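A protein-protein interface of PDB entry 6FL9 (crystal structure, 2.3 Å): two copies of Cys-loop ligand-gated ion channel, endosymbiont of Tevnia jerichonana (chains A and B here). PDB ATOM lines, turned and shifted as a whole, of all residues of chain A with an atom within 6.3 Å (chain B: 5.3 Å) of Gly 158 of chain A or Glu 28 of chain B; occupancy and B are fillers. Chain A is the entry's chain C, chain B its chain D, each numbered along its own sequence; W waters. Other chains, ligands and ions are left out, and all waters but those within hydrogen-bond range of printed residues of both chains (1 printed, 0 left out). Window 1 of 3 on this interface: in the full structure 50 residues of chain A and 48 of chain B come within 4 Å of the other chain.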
ATOM      1  N   ASP A  18       1.178  -6.128 -22.292  1.00  0.00           N
ATOM      2  CA  ASP A  18       0.363  -5.137 -21.587  1.00  0.00           C
ATOM      3  C   ASP A  18      -1.063  -5.198 -22.011  1.00  0.00           C
ATOM      4  O   ASP A  18      -1.980  -4.992 -21.193  1.00  0.00           O
ATOM      5  CB  ASP A  18       0.897  -3.716 -21.826  1.00  0.00           C
ATOM      6  CG  ASP A  18       2.292  -3.459 -21.265  1.00  0.00           C
ATOM      7  OD1 ASP A  18       2.434  -3.401 -20.018  1.00  0.00           O
ATOM      8  OD2 ASP A  18       3.238  -3.286 -22.079  1.00  0.00           O
ATOM      9  N   GLN A  19      -1.261  -5.437 -23.324  1.00  0.00           N
ATOM     10  CA  GLN A  19      -2.548  -5.441 -23.960  1.00  0.00           C
ATOM     11  C   GLN A  19      -2.664  -6.567 -24.957  1.00  0.00           C
ATOM     12  O   GLN A  19      -1.669  -6.924 -25.592  1.00  0.00           O
ATOM     13  CB  GLN A  19      -2.723  -4.119 -24.737  1.00  0.00           C
ATOM     14  CG  GLN A  19      -2.692  -2.847 -23.925  1.00  0.00           C
ATOM     15  CD  GLN A  19      -2.822  -1.628 -24.784  1.00  0.00           C
ATOM     16  OE1 GLN A  19      -3.658  -1.570 -25.673  1.00  0.00           O
ATOM     17  NE2 GLN A  19      -2.003  -0.622 -24.527  1.00  0.00           N
ATOM     18  N   ILE A  20      -3.909  -7.086 -25.117  1.00  0.00           N
ATOM     19  CA  ILE A  20      -4.383  -7.996 -26.172  1.00  0.00           C
ATOM     20  C   ILE A  20      -5.294  -7.100 -26.987  1.00  0.00           C
ATOM     21  O   ILE A  20      -6.411  -6.822 -26.560  1.00  0.00           O
ATOM     22  CB  ILE A  20      -5.053  -9.313 -25.719  1.00  0.00           C
ATOM     23  CG1 ILE A  20      -4.033 -10.242 -25.003  1.00  0.00           C
ATOM     24  CG2 ILE A  20      -5.580 -10.022 -26.945  1.00  0.00           C
ATOM     25  CD1 ILE A  20      -4.554 -11.718 -24.577  1.00  0.00           C
ATOM     26  N   ASP A 155      -2.550  -6.728 -16.167  1.00  0.00           N
ATOM     27  CA  ASP A 155      -3.876  -6.912 -15.566  1.00  0.00           C
ATOM     28  C   ASP A 155      -4.981  -6.024 -16.171  1.00  0.00           C
ATOM     29  O   ASP A 155      -6.109  -5.987 -15.660  1.00  0.00           O
ATOM     30  CB  ASP A 155      -3.783  -6.761 -14.051  1.00  0.00           C
ATOM     31  CG  ASP A 155      -3.159  -7.981 -13.395  1.00  0.00           C
ATOM     32  OD1 ASP A 155      -3.790  -9.074 -13.445  1.00  0.00           O
ATOM     33  OD2 ASP A 155      -2.044  -7.848 -12.831  1.00  0.00           O
ATOM     34  N   GLN A 156      -4.677  -5.386 -17.314  1.00  0.00           N
ATOM     35  CA  GLN A 156      -5.631  -4.594 -18.091  1.00  0.00           C
ATOM     36  C   GLN A 156      -5.459  -4.906 -19.570  1.00  0.00           C
ATOM     37  O   GLN A 156      -5.399  -3.982 -20.378  1.00  0.00           O
ATOM     38  CB  GLN A 156      -5.502  -3.095 -17.814  1.00  0.00           C
ATOM     39  CG  GLN A 156      -6.478  -2.595 -16.773  1.00  0.00           C
ATOM     40  CD  GLN A 156      -6.697  -1.103 -16.841  1.00  0.00           C
ATOM     41  OE1 GLN A 156      -5.758  -0.293 -16.984  1.00  0.00           O
ATOM     42  NE2 GLN A 156      -7.950  -0.698 -16.668  1.00  0.00           N
ATOM     43  N   LEU A 157      -5.388  -6.223 -19.920  1.00  0.00           N
ATOM     44  CA  LEU A 157      -5.223  -6.766 -21.290  1.00  0.00           C
ATOM     45  C   LEU A 157      -6.231  -6.272 -22.296  1.00  0.00           C
ATOM     46  O   LEU A 157      -5.946  -6.297 -23.492  1.00  0.00           O
ATOM     47  CB  LEU A 157      -5.206  -8.311 -21.297  1.00  0.00           C
ATOM     48  CG  LEU A 157      -4.182  -9.006 -20.377  1.00  0.00           C
ATOM     49  CD1 LEU A 157      -4.440 -10.492 -20.346  1.00  0.00           C
ATOM     50  CD2 LEU A 157      -2.730  -8.724 -20.801  1.00  0.00           C
ATOM     51  N   GLY A 158      -7.382  -5.832 -21.796  1.00  0.00           N
ATOM     52  CA  GLY A 158      -8.526  -5.346 -22.578  1.00  0.00           C
ATOM     53  C   GLY A 158      -9.253  -6.326 -23.486  1.00  0.00           C
ATOM     54  O   GLY A 158      -9.983  -5.893 -24.394  1.00  0.00           O
ATOM     55  N   GLU A 159      -9.074  -7.649 -23.254  1.00  0.00           N
ATOM     56  CA  GLU A 159      -9.762  -8.683 -24.035  1.00  0.00           C
ATOM     57  C   GLU A 159     -11.024  -9.113 -23.264  1.00  0.00           C
ATOM     58  O   GLU A 159     -10.954  -9.364 -22.050  1.00  0.00           O
ATOM     59  CB  GLU A 159      -8.814  -9.844 -24.428  1.00  0.00           C
ATOM     60  CG  GLU A 159      -9.435 -10.963 -25.244  1.00  0.00           C
ATOM     61  CD  GLU A 159     -10.132 -10.571 -26.528  1.00  0.00           C
ATOM     62  OE1 GLU A 159      -9.626  -9.685 -27.259  1.00  0.00           O
ATOM     63  OE2 GLU A 159     -11.175 -11.192 -26.818  1.00  0.00           O
ATOM     64  N   GLU A 160     -12.192  -9.116 -23.973  1.00  0.00           N
ATOM     65  CA  GLU A 160     -13.502  -9.397 -23.394  1.00  0.00           C
ATOM     66  C   GLU A 160     -14.033 -10.799 -23.612  1.00  0.00           C
ATOM     67  O   GLU A 160     -14.839 -11.267 -22.783  1.00  0.00           O
ATOM     68  CB  GLU A 160     -14.558  -8.376 -23.880  1.00  0.00           C
ATOM     69  CG  GLU A 160     -14.578  -7.075 -23.095  1.00  0.00           C
ATOM     70  CD  GLU A 160     -15.284  -7.006 -21.749  1.00  0.00           C
ATOM     71  OE1 GLU A 160     -15.622  -8.068 -21.174  1.00  0.00           O
ATOM     72  OE2 GLU A 160     -15.510  -5.869 -21.271  1.00  0.00           O
ATOM     73  N   ASN B  24     -14.214   3.227 -30.950  1.00  0.00           N
ATOM     74  CA  ASN B  24     -14.544   1.924 -31.511  1.00  0.00           C
ATOM     75  C   ASN B  24     -14.813   1.019 -30.326  1.00  0.00           C
ATOM     76  O   ASN B  24     -13.874   0.520 -29.691  1.00  0.00           O
ATOM     77  CB  ASN B  24     -13.422   1.414 -32.432  1.00  0.00           C
ATOM     78  CG  ASN B  24     -13.646   0.049 -33.039  1.00  0.00           C
ATOM     79  OD1 ASN B  24     -14.105  -0.909 -32.407  1.00  0.00           O
ATOM     80  ND2 ASN B  24     -13.227  -0.102 -34.256  1.00  0.00           N
ATOM     81  N   GLN B  25     -16.115   0.851 -29.993  1.00  0.00           N
ATOM     82  CA  GLN B  25     -16.516   0.076 -28.834  1.00  0.00           C
ATOM     83  C   GLN B  25     -16.410  -1.431 -29.070  1.00  0.00           C
ATOM     84  O   GLN B  25     -16.400  -2.188 -28.101  1.00  0.00           O
ATOM     85  CB  GLN B  25     -17.912   0.501 -28.369  1.00  0.00           C
ATOM     86  CG  GLN B  25     -18.998   0.311 -29.427  1.00  0.00           C
ATOM     87  CD  GLN B  25     -20.377   0.671 -28.943  1.00  0.00           C
ATOM     88  OE1 GLN B  25     -20.592   1.019 -27.787  1.00  0.00           O
ATOM     89  NE2 GLN B  25     -21.356   0.577 -29.822  1.00  0.00           N
ATOM     90  N   LYS B  26     -16.336  -1.877 -30.345  1.00  0.00           N
ATOM     91  CA  LYS B  26     -16.189  -3.314 -30.620  1.00  0.00           C
ATOM     92  C   LYS B  26     -14.785  -3.786 -30.224  1.00  0.00           C
ATOM     93  O   LYS B  26     -14.650  -4.888 -29.685  1.00  0.00           O
ATOM     94  CB  LYS B  26     -16.492  -3.666 -32.087  1.00  0.00           C
ATOM     95  CG  LYS B  26     -16.473  -5.167 -32.362  1.00  0.00           C
ATOM     96  CD  LYS B  26     -17.307  -5.569 -33.560  1.00  0.00           C
ATOM     97  CE  LYS B  26     -17.397  -7.074 -33.678  1.00  0.00           C
ATOM     98  NZ  LYS B  26     -18.442  -7.640 -32.775  1.00  0.00           N
ATOM     99  N   GLU B  27     -13.769  -2.938 -30.476  1.00  0.00           N
ATOM    100  CA  GLU B  27     -12.333  -3.184 -30.161  1.00  0.00           C
ATOM    101  C   GLU B  27     -11.881  -2.561 -28.819  1.00  0.00           C
ATOM    102  O   GLU B  27     -10.750  -2.805 -28.380  1.00  0.00           O
ATOM    103  CB  GLU B  27     -11.425  -2.720 -31.309  1.00  0.00           C
ATOM    104  CG  GLU B  27     -11.750  -3.385 -32.645  1.00  0.00           C
ATOM    105  CD  GLU B  27     -10.818  -3.084 -33.809  1.00  0.00           C
ATOM    106  OE1 GLU B  27     -10.112  -2.046 -33.773  1.00  0.00           O
ATOM    107  OE2 GLU B  27     -10.818  -3.879 -34.778  1.00  0.00           O
ATOM    108  N   GLU B  28     -12.769  -1.779 -28.168  1.00  0.00           N
ATOM    109  CA  GLU B  28     -12.555  -1.090 -26.883  1.00  0.00           C
ATOM    110  C   GLU B  28     -11.299  -0.249 -26.875  1.00  0.00           C
ATOM    111  O   GLU B  28     -10.344  -0.471 -26.101  1.00  0.00           O
ATOM    112  CB  GLU B  28     -12.601  -2.045 -25.684  1.00  0.00           C
ATOM    113  CG  GLU B  28     -13.952  -2.693 -25.466  1.00  0.00           C
ATOM    114  CD  GLU B  28     -13.912  -3.811 -24.450  1.00  0.00           C
ATOM    115  OE1 GLU B  28     -12.895  -4.545 -24.409  1.00  0.00           O
ATOM    116  OE2 GLU B  28     -14.902  -3.958 -23.697  1.00  0.00           O
ATOM    117  N   ASN B  29     -11.297   0.705 -27.805  1.00  0.00           N
ATOM    118  CA  ASN B  29     -10.232   1.672 -27.999  1.00  0.00           C
ATOM    119  C   ASN B  29     -10.837   2.958 -28.528  1.00  0.00           C
ATOM    120  O   ASN B  29     -12.027   2.994 -28.884  1.00  0.00           O
ATOM    121  CB  ASN B  29      -9.175   1.113 -28.931  1.00  0.00           C
ATOM    122  CG  ASN B  29      -9.552   0.928 -30.370  1.00  0.00           C
ATOM    123  OD1 ASN B  29     -10.152   1.812 -31.047  1.00  0.00           O
ATOM    124  ND2 ASN B  29      -8.995  -0.155 -30.907  1.00  0.00           N
ATOM    125  N   PHE B  30     -10.052   4.010 -28.549  1.00  0.00           N
ATOM    126  CA  PHE B  30     -10.486   5.300 -29.062  1.00  0.00           C
ATOM    127  C   PHE B  30      -9.307   5.986 -29.745  1.00  0.00           C
ATOM    128  O   PHE B  30      -8.164   5.641 -29.481  1.00  0.00           O
ATOM    129  CB  PHE B  30     -11.080   6.173 -27.946  1.00  0.00           C
ATOM    130  CG  PHE B  30     -10.132   6.617 -26.861  1.00  0.00           C
ATOM    131  CD1 PHE B  30      -9.715   5.730 -25.872  1.00  0.00           C
ATOM    132  CD2 PHE B  30      -9.725   7.940 -26.776  1.00  0.00           C
ATOM    133  CE1 PHE B  30      -8.857   6.147 -24.845  1.00  0.00           C
ATOM    134  CE2 PHE B  30      -8.855   8.354 -25.757  1.00  0.00           C
ATOM    135  CZ  PHE B  30      -8.436   7.453 -24.796  1.00  0.00           C
ATOM    136  N   GLN B  84      -1.844   2.238 -28.682  1.00  0.00           N
ATOM    137  CA  GLN B  84      -2.014   1.099 -29.576  1.00  0.00           C
ATOM    138  C   GLN B  84      -1.621   1.462 -31.016  1.00  0.00           C
ATOM    139  O   GLN B  84      -2.110   2.475 -31.568  1.00  0.00           O
ATOM    140  CB  GLN B  84      -3.468   0.648 -29.570  1.00  0.00           C
ATOM    141  CG  GLN B  84      -3.963  -0.074 -28.316  1.00  0.00           C
ATOM    142  CD  GLN B  84      -5.365  -0.644 -28.510  1.00  0.00           C
ATOM    143  OE1 GLN B  84      -5.990  -0.538 -29.580  1.00  0.00           O
ATOM    144  NE2 GLN B  84      -5.866  -1.329 -27.499  1.00  0.00           N
ATOM    145  N   PHE B 112      -5.776   4.575 -28.569  1.00  0.00           N
ATOM    146  CA  PHE B 112      -5.496   4.218 -27.191  1.00  0.00           C
ATOM    147  C   PHE B 112      -6.503   3.185 -26.710  1.00  0.00           C
ATOM    148  O   PHE B 112      -7.688   3.278 -27.024  1.00  0.00           O
ATOM    149  CB  PHE B 112      -5.540   5.464 -26.291  1.00  0.00           C
ATOM    150  CG  PHE B 112      -4.476   6.488 -26.620  1.00  0.00           C
ATOM    151  CD1 PHE B 112      -3.215   6.424 -26.027  1.00  0.00           C
ATOM    152  CD2 PHE B 112      -4.720   7.497 -27.550  1.00  0.00           C
ATOM    153  CE1 PHE B 112      -2.218   7.342 -26.368  1.00  0.00           C
ATOM    154  CE2 PHE B 112      -3.714   8.412 -27.892  1.00  0.00           C
ATOM    155  CZ  PHE B 112      -2.476   8.336 -27.291  1.00  0.00           C
ATOM    156  N   GLN B 113      -6.026   2.226 -25.924  1.00  0.00           N
ATOM    157  CA  GLN B 113      -6.846   1.211 -25.299  1.00  0.00           C
ATOM    158  C   GLN B 113      -7.862   1.882 -24.364  1.00  0.00           C
ATOM    159  O   GLN B 113      -7.531   2.814 -23.628  1.00  0.00           O
ATOM    160  CB  GLN B 113      -5.961   0.272 -24.489  1.00  0.00           C
ATOM    161  CG  GLN B 113      -6.615  -1.074 -24.239  1.00  0.00           C
ATOM    162  CD  GLN B 113      -6.045  -1.773 -23.036  1.00  0.00           C
ATOM    163  OE1 GLN B 113      -5.512  -1.164 -22.137  1.00  0.00           O
ATOM    164  NE2 GLN B 113      -6.180  -3.061 -22.947  1.00  0.00           N
ATOM    165  N   ALA B 114      -9.103   1.413 -24.433  1.00  0.00           N
ATOM    166  CA  ALA B 114     -10.219   1.832 -23.572  1.00  0.00           C
ATOM    167  C   ALA B 114     -10.610   0.595 -22.726  1.00  0.00           C
ATOM    168  O   ALA B 114     -11.502  -0.162 -23.111  1.00  0.00           O
ATOM    169  CB  ALA B 114     -11.394   2.330 -24.417  1.00  0.00           C
ATOM    170  N   PRO B 115      -9.851   0.291 -21.642  1.00  0.00           N
ATOM    171  CA  PRO B 115     -10.130  -0.941 -20.882  1.00  0.00           C
ATOM    172  C   PRO B 115     -11.201  -0.809 -19.803  1.00  0.00           C
ATOM    173  O   PRO B 115     -11.563  -1.814 -19.194  1.00  0.00           O
ATOM    174  CB  PRO B 115      -8.756  -1.333 -20.317  1.00  0.00           C
ATOM    175  CG  PRO B 115      -7.903  -0.093 -20.430  1.00  0.00           C
ATOM    176  CD  PRO B 115      -8.675   0.996 -21.095  1.00  0.00           C
ATOM    177  N   PHE B 117     -14.337  -0.015 -20.341  1.00  0.00           N
ATOM    178  CA  PHE B 117     -15.624  -0.275 -20.983  1.00  0.00           C
ATOM    179  C   PHE B 117     -16.559  -1.236 -20.233  1.00  0.00           C
ATOM    180  O   PHE B 117     -16.270  -2.430 -20.121  1.00  0.00           O
ATOM    181  CB  PHE B 117     -15.433  -0.749 -22.416  1.00  0.00           C
ATOM    182  CG  PHE B 117     -15.652   0.331 -23.445  1.00  0.00           C
ATOM    183  CD1 PHE B 117     -16.916   0.890 -23.636  1.00  0.00           C
ATOM    184  CD2 PHE B 117     -14.609   0.758 -24.260  1.00  0.00           C
ATOM    185  CE1 PHE B 117     -17.121   1.879 -24.606  1.00  0.00           C
ATOM    186  CE2 PHE B 117     -14.821   1.736 -25.245  1.00  0.00           C
ATOM    187  CZ  PHE B 117     -16.072   2.290 -25.408  1.00  0.00           C
ATOM    188  N   PHE B 119     -20.398  -2.359 -20.600  1.00  0.00           N
ATOM    189  CA  PHE B 119     -21.599  -2.366 -21.450  1.00  0.00           C
ATOM    190  C   PHE B 119     -22.868  -2.844 -20.764  1.00  0.00           C
ATOM    191  O   PHE B 119     -23.930  -2.849 -21.406  1.00  0.00           O
ATOM    192  CB  PHE B 119     -21.347  -3.171 -22.710  1.00  0.00           C
ATOM    193  CG  PHE B 119     -20.265  -2.631 -23.600  1.00  0.00           C
ATOM    194  CD1 PHE B 119     -20.513  -1.561 -24.457  1.00  0.00           C
ATOM    195  CD2 PHE B 119     -19.009  -3.233 -23.640  1.00  0.00           C
ATOM    196  CE1 PHE B 119     -19.523  -1.104 -25.339  1.00  0.00           C
ATOM    197  CE2 PHE B 119     -18.036  -2.786 -24.530  1.00  0.00           C
ATOM    198  CZ  PHE B 119     -18.303  -1.731 -25.380  1.00  0.00           C
ATOM    199  N   PRO B 248     -18.377  -5.975 -28.429  1.00  0.00           N
ATOM    200  CA  PRO B 248     -17.483  -7.138 -28.442  1.00  0.00           C
ATOM    201  C   PRO B 248     -18.273  -8.378 -28.007  1.00  0.00           C
ATOM    202  O   PRO B 248     -19.431  -8.273 -27.596  1.00  0.00           O
ATOM    203  CB  PRO B 248     -16.387  -6.762 -27.440  1.00  0.00           C
ATOM    204  CG  PRO B 248     -16.680  -5.369 -27.018  1.00  0.00           C
ATOM    205  CD  PRO B 248     -18.095  -5.123 -27.255  1.00  0.00           C
ATOM    206  N   LEU B 250     -18.825 -10.125 -25.473  1.00  0.00           N
ATOM    207  CA  LEU B 250     -18.789 -10.004 -24.024  1.00  0.00           C
ATOM    208  C   LEU B 250     -19.107 -11.313 -23.306  1.00  0.00           C
ATOM    209  O   LEU B 250     -19.761 -12.199 -23.853  1.00  0.00           O
ATOM    210  CB  LEU B 250     -19.797  -8.906 -23.587  1.00  0.00           C
ATOM    211  CG  LEU B 250     -19.575  -7.508 -24.182  1.00  0.00           C
ATOM    212  CD1 LEU B 250     -20.755  -6.607 -23.916  1.00  0.00           C
ATOM    213  CD2 LEU B 250     -18.329  -6.877 -23.634  1.00  0.00           C
HETATM  214  O   HOH W   1      -6.359  -4.337 -25.345  1.00  0.00           O
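Water W1 lies within hydrogen-bond range of the side-chain amide nitrogen (NE2) of Gln 113 of chain B (2.7 Å), the backbone carbonyl oxygen (O) of Leu 157 of chain A (2.7 Å) and the backbone carbonyl oxygen (O) of Ile 20 of chain A (2.8 Å).
Of the printed residues of chain B, Gln 156 of chain A touches Gln 113 and Pro 115. Of the printed residues of chain B, Leu 157 of chain A touches Gln 113 (3.3 Å). Glu 28 of chain B touches two residues of chain A. Printed residues of chain A within 4 Å of Phe 117 of chain B: Glu 160. The nearest residue of chain B that does not touch Gly 158 of chain A is Pro 115 of chain B (4.6 Å). The nearest residue of chain A that does not touch Glu 28 of chain B is Glu 159 of chain A (5.1 Å). The nearest printed residue of chain A that does not touch Pro 115 of chain B is Gly 158 of chain A (4.6 Å).
Of the 9 printed residues of chain A, 5 touch a printed residue of chain B. Printed residues of chain A that touch a printed residue of chain B: Gln 19, Gln 156, Leu 157, Gly 158 and Glu 160. Among the printed residues, no Asp or Glu carboxylate lies within 4 Å of a Lys or Arg side-chain nitrogen of the other chain.
No position is printed for both chains. Of the 10 pairs that touch across the chains among the printed residues, none has its exchanged pair printed and touching as well.
O of Gly 158 of chain A sits close to OE1 of Glu 28 of chain B (3.2 Å). The backbone carbonyl oxygen (O) of Gln 156 of chain A is in hydrogen-bond range of the side-chain amide nitrogen (NE2) of Gln 113 of chain B (2.8 Å). O of Leu 157 of chain A lies close to NE2 of Gln 113 of chain B (3.3 Å). The side-chain amide oxygen (OE1) of Gln 19 of chain A sits at hydrogen-bond distance from the side-chain amide nitrogen (NE2) of Gln 84 of chain B (2.9 Å). The side-chain carboxylate of Glu 160 of chain A lies close to the side-chain carboxylate of Glu 28 of chain B (3.1 Å). NE2 of Gln 113 of chain B lies close to N of Gly 158 of chain A (3.2 Å).
The backbone carbonyl oxygen of Glu 28 of chain B is in hydrogen-bond range of the backbone NH of Ala 114 of chain B (2.8 Å). The side-chain amide nitrogen (ND2) of Asn 29 of chain B sits at hydrogen-bond distance from the side-chain amide oxygen (OE1) of Gln 84 of chain B (3.3 Å). The backbone carbonyl oxygen of Leu 157 of chain A sits at hydrogen-bond distance from the backbone NH of Ile 20 of chain A, at 2.7 Å.
Among the printed residues, pairs that only touch across the chains: Gln 19 of chain A with Gln 113 of chain B (3.2 Å), Glu 160 of chain A with Leu 250 of chain B (3.6 Å), Glu 160 of chain A with Phe 117 of chain B (3.7 Å) and Gln 156 of chain A with Pro 115 of chain B (3.8 Å).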
